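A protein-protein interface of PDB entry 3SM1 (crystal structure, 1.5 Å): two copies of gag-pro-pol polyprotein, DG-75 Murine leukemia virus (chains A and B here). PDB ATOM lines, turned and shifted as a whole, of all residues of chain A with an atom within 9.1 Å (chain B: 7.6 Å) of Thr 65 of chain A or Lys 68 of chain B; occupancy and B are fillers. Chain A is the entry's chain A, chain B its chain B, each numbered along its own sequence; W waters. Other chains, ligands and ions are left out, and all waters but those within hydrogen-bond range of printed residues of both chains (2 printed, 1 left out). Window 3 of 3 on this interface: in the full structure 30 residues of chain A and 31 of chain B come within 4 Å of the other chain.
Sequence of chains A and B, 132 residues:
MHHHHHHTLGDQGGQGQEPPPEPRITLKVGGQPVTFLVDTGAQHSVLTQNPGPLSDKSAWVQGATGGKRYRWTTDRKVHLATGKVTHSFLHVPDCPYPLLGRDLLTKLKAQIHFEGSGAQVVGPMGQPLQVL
N of Cys 95 of chain B lies within hydrogen-bond range of O of Ala 64 of chain A, 3.3 Å away.
OG1 of Thr 65 of chain B sits close to O of Gly 66 of chain A (3.5 Å).
The side-chain hydroxyl (OG1) of Thr 65 of chain A is in hydrogen-bond range of the backbone carbonyl oxygen (O) of Gly 66 of chain B, at 2.9 Å.
O of Asp 94 of chain A lies close to OE1 of Gln 62 of chain B, 3.1 Å away.
N of Ala 59 of chain B is in hydrogen-bond range of O of Tyr 70 of chain B (2.8 Å).
NZ of Lys 68 of chain A is in salt-bridge range of OD2 of Asp 94 of chain A.
The side-chain hydroxyl (OH) of Tyr 70 of chain B is in hydrogen-bond range of the side-chain carboxylate (OD2) of Asp 94 of chain B (2.7 Å).
The side-chain amino group (NZ) of Lys 68 of chain B lies within salt-bridge range of the side-chain carboxylate (OD2) of Asp 94 of chain B (3.2 Å).
The side-chain amide oxygen (OE1) of Gln 62 of chain B sits close to the backbone carbonyl oxygen (O) of Gly 66 of chain B.
The backbone carbonyl oxygen of Lys 68 of chain B lies within hydrogen-bond range of the backbone NH of Val 61 of chain B, 2.8 Å away.
Among the printed residues, merely in contact across the chains: Val 61 of chain A with Thr 65 of chain B, Gln 62 of chain A with Asp 94 of chain B, Gln 62 of chain A with Pro 96 of chain B, Ala 64 of chain A with Val 92 of chain B, Ala 64 of chain A with Asp 94 of chain B, Thr 65 of chain A with Val 61 of chain B, Thr 65 of chain A with Gly 63 of chain B, Thr 65 of chain A with Lys 68 of chain B, Thr 65 of chain A with Tyr 70 of chain B, Thr 65 of chain A with Asp 94 of chain B, Gly 67 of chain A with Thr 65 of chain B, Tyr 70 of chain A with Thr 65 of chain B, Asp 94 of chain A with Ala 64 of chain B, Asp 94 of chain A with Thr 65 of chain B, Pro 96 of chain A with Gln 62 of chain B and Pro 96 of chain A with Gly 63 of chain B.
Thr 65 of chain A touches just these residues of chain B: Val 61, Gly 63, Gly 66, Lys 68, Tyr 70 and Asp 94.
Of the printed residues of chain B, Asp 94 of chain A touches Gln 62, Ala 64 and Thr 65.
Of the printed residues of chain B, Pro 96 of chain A touches Gln 62 and Gly 63.
Trp 60 of chain B touches none of the printed residues of chain A.
Val 61 of chain B touches just one residue of chain A: Thr 65 (3.8 Å).
Printed residues of chain A within 4 Å of Gln 62 of chain B: Asp 94 and Pro 96.
Of the printed residues of chain A, Ala 64 of chain B touches Asp 94 (3.4 Å).
No residue of chain A comes within 4 Å of Gly 67 of chain B.
Lys 68 of chain B touches one residue of chain A.
Of the printed residues of chain A, Tyr 70 of chain B touches Thr 65.
The nearest residue of chain B that does not touch Thr 65 of chain A is Gly 67 of chain B (4.1 Å).
The nearest printed residue of chain A that does not touch Val 92 of chain B is Thr 65 of chain A (5.0 Å).
Hydrophobic or aromatic side chains of chain A that line the printed part of chain B: Ala 64, Tyr 70 and Pro 96.
Of the 18 printed residues of chain B, 12 touch a printed residue of chain A.
Hydrophobic or aromatic side chains of chain B that line the printed part of chain A: Val 61, Tyr 70, Val 92 and Pro 96.
Among the printed residues, 20 pairs touch across the chains.
Among the printed residues, no Asp or Glu carboxylate lies within 4 Å of a Lys or Arg side-chain nitrogen of the other chain.
Thr 65 of chain A touches Gly 63 of chain B, but with the chains exchanged Gly 63 of chain A does not touch Thr 65 of chain B (4.1 Å).
Thr 65 of chain A touches Tyr 70 of chain B, and with the chains exchanged Tyr 70 of chain A touches Thr 65 of chain B.
Thr 65 of chain A touches Asp 94 of chain B, and with the chains exchanged Asp 94 of chain A touches Thr 65 of chain B.
Pro 96 of chain A touches Gly 63 of chain B, but with the chains exchanged Gly 63 of chain A does not touch Pro 96 of chain B (4.2 Å).
Water W2 lies within hydrogen-bond range of OG1 of Thr 65 of chain A (2.7 Å), OG1 of Thr 65 of chain B (2.8 Å) and N of Ala 64 of chain B (3.5 Å).
Water W1 bridges the backbone NH of Ala 64 of chain A (2.8 Å) and the backbone NH of Ala 64 of chain B (2.9 Å).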
ATOM      1  N   VAL A  61      32.321 -32.223  14.600  1.00  0.00           N
ATOM      2  CA  VAL A  61      32.158 -31.399  13.398  1.00  0.00           C
ATOM      3  C   VAL A  61      32.648 -30.002  13.745  1.00  0.00           C
ATOM      4  O   VAL A  61      32.093 -29.386  14.638  1.00  0.00           O
ATOM      5  CB  VAL A  61      30.676 -31.329  12.999  1.00  0.00           C
ATOM      6  CG1 VAL A  61      30.415 -30.368  11.820  1.00  0.00           C
ATOM      7  CG2 VAL A  61      30.214 -32.736  12.581  1.00  0.00           C
ATOM      8  N   GLN A  62      33.636 -29.517  12.989  1.00  0.00           N
ATOM      9  CA  GLN A  62      34.039 -28.116  13.096  1.00  0.00           C
ATOM     10  C   GLN A  62      33.328 -27.313  12.036  1.00  0.00           C
ATOM     11  O   GLN A  62      33.487 -27.591  10.840  1.00  0.00           O
ATOM     12  CB  GLN A  62      35.546 -27.996  12.936  1.00  0.00           C
ATOM     13  CG  GLN A  62      35.956 -26.495  13.010  1.00  0.00           C
ATOM     14  CD  GLN A  62      37.424 -26.228  12.839  1.00  0.00           C
ATOM     15  OE1 GLN A  62      37.916 -25.217  13.342  1.00  0.00           O
ATOM     16  NE2 GLN A  62      38.109 -27.062  12.113  1.00  0.00           N
ATOM     17  N   GLY A  63      32.581 -26.314  12.496  1.00  0.00           N
ATOM     18  CA  GLY A  63      31.955 -25.353  11.595  1.00  0.00           C
ATOM     19  C   GLY A  63      32.747 -24.051  11.523  1.00  0.00           C
ATOM     20  O   GLY A  63      33.823 -23.914  12.124  1.00  0.00           O
ATOM     21  N   ALA A  64      32.195 -23.077  10.821  1.00  0.00           N
ATOM     22  CA  ALA A  64      32.897 -21.797  10.720  1.00  0.00           C
ATOM     23  C   ALA A  64      32.922 -21.037  12.042  1.00  0.00           C
ATOM     24  O   ALA A  64      33.780 -20.181  12.231  1.00  0.00           O
ATOM     25  CB  ALA A  64      32.261 -20.949   9.610  1.00  0.00           C
ATOM     26  N   THR A  65      32.000 -21.332  12.969  1.00  0.00           N
ATOM     27  CA  THR A  65      31.805 -20.531  14.171  1.00  0.00           C
ATOM     28  C   THR A  65      32.067 -21.305  15.462  1.00  0.00           C
ATOM     29  O   THR A  65      31.984 -20.748  16.589  1.00  0.00           O
ATOM     30  CB  THR A  65      30.386 -19.904  14.239  1.00  0.00           C
ATOM     31  OG1 THR A  65      29.431 -20.967  14.380  1.00  0.00           O
ATOM     32  CG2 THR A  65      30.049 -19.129  12.958  1.00  0.00           C
ATOM     33  N   GLY A  66      32.416 -22.583  15.328  1.00  0.00           N
ATOM     34  CA  GLY A  66      32.579 -23.417  16.529  1.00  0.00           C
ATOM     35  C   GLY A  66      32.542 -24.860  16.114  1.00  0.00           C
ATOM     36  O   GLY A  66      32.730 -25.150  14.971  1.00  0.00           O
ATOM     37  N   GLY A  67      32.265 -25.745  17.051  1.00  0.00           N
ATOM     38  CA  GLY A  67      32.261 -27.162  16.757  1.00  0.00           C
ATOM     39  C   GLY A  67      31.395 -27.870  17.775  1.00  0.00           C
ATOM     40  O   GLY A  67      31.144 -27.360  18.874  1.00  0.00           O
ATOM     41  N   LYS A  68      30.919 -29.053  17.394  1.00  0.00           N
ATOM     42  CA  LYS A  68      30.046 -29.840  18.242  1.00  0.00           C
ATOM     43  C   LYS A  68      30.035 -31.281  17.732  1.00  0.00           C
ATOM     44  O   LYS A  68      30.398 -31.554  16.592  1.00  0.00           O
ATOM     45  CB  LYS A  68      28.633 -29.265  18.157  1.00  0.00           C
ATOM     46  CG  LYS A  68      27.770 -29.530  19.353  1.00  0.00           C
ATOM     47  CD  LYS A  68      26.676 -28.495  19.456  1.00  0.00           C
ATOM     48  CE  LYS A  68      25.380 -29.002  18.870  1.00  0.00           C
ATOM     49  NZ  LYS A  68      24.691 -30.023  19.710  1.00  0.00           N
ATOM     50  N   TYR A  70      28.071 -34.645  16.541  1.00  0.00           N
ATOM     51  CA  TYR A  70      26.800 -35.022  15.895  1.00  0.00           C
ATOM     52  C   TYR A  70      26.847 -36.479  15.487  1.00  0.00           C
ATOM     53  O   TYR A  70      27.907 -37.057  15.287  1.00  0.00           O
ATOM     54  CB  TYR A  70      26.556 -34.183  14.633  1.00  0.00           C
ATOM     55  CG  TYR A  70      26.376 -32.717  14.939  1.00  0.00           C
ATOM     56  CD1 TYR A  70      25.177 -32.221  15.412  1.00  0.00           C
ATOM     57  CD2 TYR A  70      27.453 -31.843  14.778  1.00  0.00           C
ATOM     58  CE1 TYR A  70      25.027 -30.830  15.702  1.00  0.00           C
ATOM     59  CE2 TYR A  70      27.316 -30.491  15.044  1.00  0.00           C
ATOM     60  CZ  TYR A  70      26.125 -29.998  15.500  1.00  0.00           C
ATOM     61  OH  TYR A  70      26.009 -28.650  15.764  1.00  0.00           O
ATOM     62  N   ASP A  94      21.421 -28.222  14.000  1.00  0.00           N
ATOM     63  CA  ASP A  94      21.788 -26.783  14.100  1.00  0.00           C
ATOM     64  C   ASP A  94      22.041 -26.099  12.741  1.00  0.00           C
ATOM     65  O   ASP A  94      22.109 -24.870  12.638  1.00  0.00           O
ATOM     66  CB  ASP A  94      23.036 -26.617  14.973  1.00  0.00           C
ATOM     67  CG  ASP A  94      22.832 -27.144  16.372  1.00  0.00           C
ATOM     68  OD1 ASP A  94      21.873 -26.698  17.053  1.00  0.00           O
ATOM     69  OD2 ASP A  94      23.623 -28.012  16.800  1.00  0.00           O
ATOM     70  N   PRO A  96      21.581 -24.640   8.977  1.00  0.00           N
ATOM     71  CA  PRO A  96      20.413 -23.992   8.353  1.00  0.00           C
ATOM     72  C   PRO A  96      19.780 -24.779   7.187  1.00  0.00           C
ATOM     73  O   PRO A  96      18.560 -24.719   6.973  1.00  0.00           O
ATOM     74  CB  PRO A  96      20.971 -22.650   7.848  1.00  0.00           C
ATOM     75  CG  PRO A  96      22.443 -22.700   8.007  1.00  0.00           C
ATOM     76  CD  PRO A  96      22.750 -23.743   9.046  1.00  0.00           C
ATOM     77  N   ALA B  59      28.314  -8.564  11.542  1.00  0.00           N
ATOM     78  CA  ALA B  59      27.230  -9.376  11.019  1.00  0.00           C
ATOM     79  C   ALA B  59      26.990 -10.528  11.976  1.00  0.00           C
ATOM     80  O   ALA B  59      27.930 -11.060  12.545  1.00  0.00           O
ATOM     81  CB  ALA B  59      27.607  -9.973   9.642  1.00  0.00           C
ATOM     82  N   TRP B  60      25.757 -10.983  12.087  1.00  0.00           N
ATOM     83  CA  TRP B  60      25.470 -12.252  12.680  1.00  0.00           C
ATOM     84  C   TRP B  60      25.791 -13.341  11.648  1.00  0.00           C
ATOM     85  O   TRP B  60      25.302 -13.291  10.512  1.00  0.00           O
ATOM     86  CB  TRP B  60      23.960 -12.333  12.998  1.00  0.00           C
ATOM     87  CG  TRP B  60      23.629 -13.600  13.662  1.00  0.00           C
ATOM     88  CD1 TRP B  60      23.262 -14.787  13.071  1.00  0.00           C
ATOM     89  CD2 TRP B  60      23.688 -13.848  15.065  1.00  0.00           C
ATOM     90  NE1 TRP B  60      23.079 -15.748  14.029  1.00  0.00           N
ATOM     91  CE2 TRP B  60      23.357 -15.210  15.259  1.00  0.00           C
ATOM     92  CE3 TRP B  60      23.990 -13.049  16.186  1.00  0.00           C
ATOM     93  CZ2 TRP B  60      23.274 -15.789  16.535  1.00  0.00           C
ATOM     94  CZ3 TRP B  60      23.923 -13.639  17.475  1.00  0.00           C
ATOM     95  CH2 TRP B  60      23.572 -15.003  17.621  1.00  0.00           C
ATOM     96  N   VAL B  61      26.630 -14.287  12.030  1.00  0.00           N
ATOM     97  CA  VAL B  61      27.039 -15.385  11.131  1.00  0.00           C
ATOM     98  C   VAL B  61      26.527 -16.694  11.699  1.00  0.00           C
ATOM     99  O   VAL B  61      26.851 -17.040  12.850  1.00  0.00           O
ATOM    100  CB  VAL B  61      28.564 -15.426  10.969  1.00  0.00           C
ATOM    101  CG1 VAL B  61      29.010 -16.642  10.111  1.00  0.00           C
ATOM    102  CG2 VAL B  61      29.048 -14.099  10.368  1.00  0.00           C
ATOM    103  N   GLN B  62      25.677 -17.390  10.938  1.00  0.00           N
ATOM    104  CA  GLN B  62      25.243 -18.758  11.290  1.00  0.00           C
ATOM    105  C   GLN B  62      26.086 -19.765  10.511  1.00  0.00           C
ATOM    106  O   GLN B  62      26.102 -19.748   9.273  1.00  0.00           O
ATOM    107  CB  GLN B  62      23.755 -18.951  10.963  1.00  0.00           C
ATOM    108  CG  GLN B  62      23.233 -20.405  11.148  1.00  0.00           C
ATOM    109  CD  GLN B  62      23.213 -20.910  12.598  1.00  0.00           C
ATOM    110  OE1 GLN B  62      23.511 -22.091  12.869  1.00  0.00           O
ATOM    111  NE2 GLN B  62      22.849 -20.032  13.535  1.00  0.00           N
ATOM    112  N   GLY B  63      26.816 -20.609  11.236  1.00  0.00           N
ATOM    113  CA  GLY B  63      27.606 -21.694  10.676  1.00  0.00           C
ATOM    114  C   GLY B  63      26.820 -22.982  10.853  1.00  0.00           C
ATOM    115  O   GLY B  63      25.644 -22.979  11.264  1.00  0.00           O
ATOM    116  N   ALA B  64      27.468 -24.096  10.535  1.00  0.00           N
ATOM    117  CA  ALA B  64      26.814 -25.404  10.659  1.00  0.00           C
ATOM    118  C   ALA B  64      26.427 -25.742  12.082  1.00  0.00           C
ATOM    119  O   ALA B  64      25.436 -26.438  12.295  1.00  0.00           O
ATOM    120  CB  ALA B  64      27.712 -26.487  10.086  1.00  0.00           C
ATOM    121  N   THR B  65      27.166 -25.221  13.064  1.00  0.00           N
ATOM    122  CA  THR B  65      26.984 -25.648  14.452  1.00  0.00           C
ATOM    123  C   THR B  65      26.406 -24.628  15.416  1.00  0.00           C
ATOM    124  O   THR B  65      26.133 -24.945  16.577  1.00  0.00           O
ATOM    125  CB  THR B  65      28.307 -26.257  15.002  1.00  0.00           C
ATOM    126  OG1 THR B  65      29.265 -25.202  15.201  1.00  0.00           O
ATOM    127  CG2 THR B  65      28.872 -27.294  14.024  1.00  0.00           C
ATOM    128  N   GLY B  66      26.234 -23.393  14.964  1.00  0.00           N
ATOM    129  CA  GLY B  66      25.787 -22.311  15.846  1.00  0.00           C
ATOM    130  C   GLY B  66      26.073 -20.998  15.182  1.00  0.00           C
ATOM    131  O   GLY B  66      26.528 -20.973  14.062  1.00  0.00           O
ATOM    132  N   GLY B  67      25.758 -19.914  15.866  1.00  0.00           N
ATOM    133  CA  GLY B  67      25.960 -18.573  15.319  1.00  0.00           C
ATOM    134  C   GLY B  67      26.450 -17.617  16.369  1.00  0.00           C
ATOM    135  O   GLY B  67      26.298 -17.826  17.579  1.00  0.00           O
ATOM    136  N   LYS B  68      27.107 -16.568  15.888  1.00  0.00           N
ATOM    137  CA  LYS B  68      27.443 -15.402  16.710  1.00  0.00           C
ATOM    138  C   LYS B  68      27.927 -14.319  15.764  1.00  0.00           C
ATOM    139  O   LYS B  68      27.930 -14.498  14.521  1.00  0.00           O
ATOM    140  CB  LYS B  68      28.500 -15.720  17.758  1.00  0.00           C
ATOM    141  CG  LYS B  68      29.829 -16.092  17.153  1.00  0.00           C
ATOM    142  CD  LYS B  68      30.941 -16.288  18.222  1.00  0.00           C
ATOM    143  CE  LYS B  68      31.158 -17.770  18.508  1.00  0.00           C
ATOM    144  NZ  LYS B  68      32.543 -18.041  19.009  1.00  0.00           N
ATOM    145  N   ARG B  69      28.265 -13.155  16.314  1.00  0.00           N
ATOM    146  CA  ARG B  69      28.591 -12.022  15.475  1.00  0.00           C
ATOM    147  C   ARG B  69      30.082 -11.910  15.230  1.00  0.00           C
ATOM    148  O   ARG B  69      30.904 -12.213  16.102  1.00  0.00           O
ATOM    149  CB  ARG B  69      28.112 -10.710  16.110  1.00  0.00           C
ATOM    150  CG  ARG B  69      26.594 -10.719  16.346  1.00  0.00           C
ATOM    151  CD  ARG B  69      26.128  -9.327  16.799  1.00  0.00           C
ATOM    152  NE  ARG B  69      26.198  -8.354  15.707  1.00  0.00           N
ATOM    153  CZ  ARG B  69      25.237  -8.133  14.820  1.00  0.00           C
ATOM    154  NH1 ARG B  69      24.051  -8.804  14.858  1.00  0.00           N
ATOM    155  NH2 ARG B  69      25.451  -7.213  13.896  1.00  0.00           N
ATOM    156  N   TYR B  70      30.408 -11.420  14.038  1.00  0.00           N
ATOM    157  CA  TYR B  70      31.792 -11.176  13.640  1.00  0.00           C
ATOM    158  C   TYR B  70      31.867  -9.854  12.939  1.00  0.00           C
ATOM    159  O   TYR B  70      30.918  -9.404  12.293  1.00  0.00           O
ATOM    160  CB  TYR B  70      32.267 -12.306  12.705  1.00  0.00           C
ATOM    161  CG  TYR B  70      32.329 -13.630  13.398  1.00  0.00           C
ATOM    162  CD1 TYR B  70      33.442 -13.990  14.158  1.00  0.00           C
ATOM    163  CD2 TYR B  70      31.252 -14.523  13.313  1.00  0.00           C
ATOM    164  CE1 TYR B  70      33.506 -15.224  14.801  1.00  0.00           C
ATOM    165  CE2 TYR B  70      31.325 -15.762  13.942  1.00  0.00           C
ATOM    166  CZ  TYR B  70      32.435 -16.092  14.686  1.00  0.00           C
ATOM    167  OH  TYR B  70      32.476 -17.342  15.286  1.00  0.00           O
ATOM    168  N   ARG B  71      33.051  -9.272  12.964  1.00  0.00           N
ATOM    169  CA  ARG B  71      33.260  -7.971  12.386  1.00  0.00           C
ATOM    170  C   ARG B  71      33.549  -7.980  10.889  1.00  0.00           C
ATOM    171  O   ARG B  71      34.158  -8.938  10.380  1.00  0.00           O
ATOM    172  CB  ARG B  71      34.493  -7.364  13.081  1.00  0.00           C
ATOM    173  CG  ARG B  71      34.526  -5.856  12.958  1.00  0.00           C
ATOM    174  CD  ARG B  71      33.762  -5.206  14.139  1.00  0.00           C
ATOM    175  NE  ARG B  71      34.523  -5.375  15.360  1.00  0.00           N
ATOM    176  CZ  ARG B  71      35.491  -4.544  15.784  1.00  0.00           C
ATOM    177  NH1 ARG B  71      35.822  -3.438  15.135  1.00  0.00           N
ATOM    178  NH2 ARG B  71      36.118  -4.819  16.909  1.00  0.00           N
ATOM    179  N   VAL B  92      36.489 -13.947  10.682  1.00  0.00           N
ATOM    180  CA  VAL B  92      35.973 -15.055  11.501  1.00  0.00           C
ATOM    181  C   VAL B  92      37.155 -15.891  12.022  1.00  0.00           C
ATOM    182  O   VAL B  92      37.568 -16.865  11.407  1.00  0.00           O
ATOM    183  CB  VAL B  92      34.987 -15.927  10.702  1.00  0.00           C
ATOM    184  CG1 VAL B  92      34.348 -16.946  11.641  1.00  0.00           C
ATOM    185  CG2 VAL B  92      33.891 -15.043  10.058  1.00  0.00           C
ATOM    186  N   PRO B  93      37.683 -15.536  13.193  1.00  0.00           N
ATOM    187  CA  PRO B  93      38.870 -16.239  13.685  1.00  0.00           C
ATOM    188  C   PRO B  93      38.581 -17.661  14.146  1.00  0.00           C
ATOM    189  O   PRO B  93      39.496 -18.477  14.273  1.00  0.00           O
ATOM    190  CB  PRO B  93      39.384 -15.339  14.813  1.00  0.00           C
ATOM    191  CG  PRO B  93      38.199 -14.488  15.210  1.00  0.00           C
ATOM    192  CD  PRO B  93      37.404 -14.301  13.951  1.00  0.00           C
ATOM    193  N   ASP B  94      37.311 -18.009  14.295  1.00  0.00           N
ATOM    194  CA  ASP B  94      36.917 -19.405  14.620  1.00  0.00           C
ATOM    195  C   ASP B  94      36.913 -20.325  13.403  1.00  0.00           C
ATOM    196  O   ASP B  94      36.789 -21.540  13.547  1.00  0.00           O
ATOM    197  CB  ASP B  94      35.525 -19.429  15.265  1.00  0.00           C
ATOM    198  CG  ASP B  94      35.500 -18.675  16.569  1.00  0.00           C
ATOM    199  OD1 ASP B  94      36.305 -19.030  17.449  1.00  0.00           O
ATOM    200  OD2 ASP B  94      34.710 -17.727  16.732  1.00  0.00           O
ATOM    201  N   CYS B  95      37.081 -19.756  12.207  1.00  0.00           N
ATOM    202  CA  CYS B  95      36.988 -20.555  10.980  1.00  0.00           C
ATOM    203  C   CYS B  95      38.408 -21.047  10.647  1.00  0.00           C
ATOM    204  O   CYS B  95      39.379 -20.304  10.793  1.00  0.00           O
ATOM    205  CB  CYS B  95      36.443 -19.660   9.894  1.00  0.00           C
ATOM    206  SG  CYS B  95      36.024 -20.525   8.391  1.00  0.00           S
ATOM    207  N   PRO B  96      38.565 -22.330  10.263  1.00  0.00           N
ATOM    208  CA  PRO B  96      39.934 -22.853  10.083  1.00  0.00           C
ATOM    209  C   PRO B  96      40.637 -22.354   8.821  1.00  0.00           C
ATOM    210  O   PRO B  96      41.862 -22.333   8.786  1.00  0.00           O
ATOM    211  CB  PRO B  96      39.717 -24.384  10.024  1.00  0.00           C
ATOM    212  CG  PRO B  96      38.301 -24.540   9.551  1.00  0.00           C
ATOM    213  CD  PRO B  96      37.537 -23.388  10.177  1.00  0.00           C
HETATM  214  O   HOH W   1      29.962 -23.705   9.168  1.00  0.00           O
HETATM  215  O   HOH W   2      29.597 -23.352  13.170  1.00  0.00           O
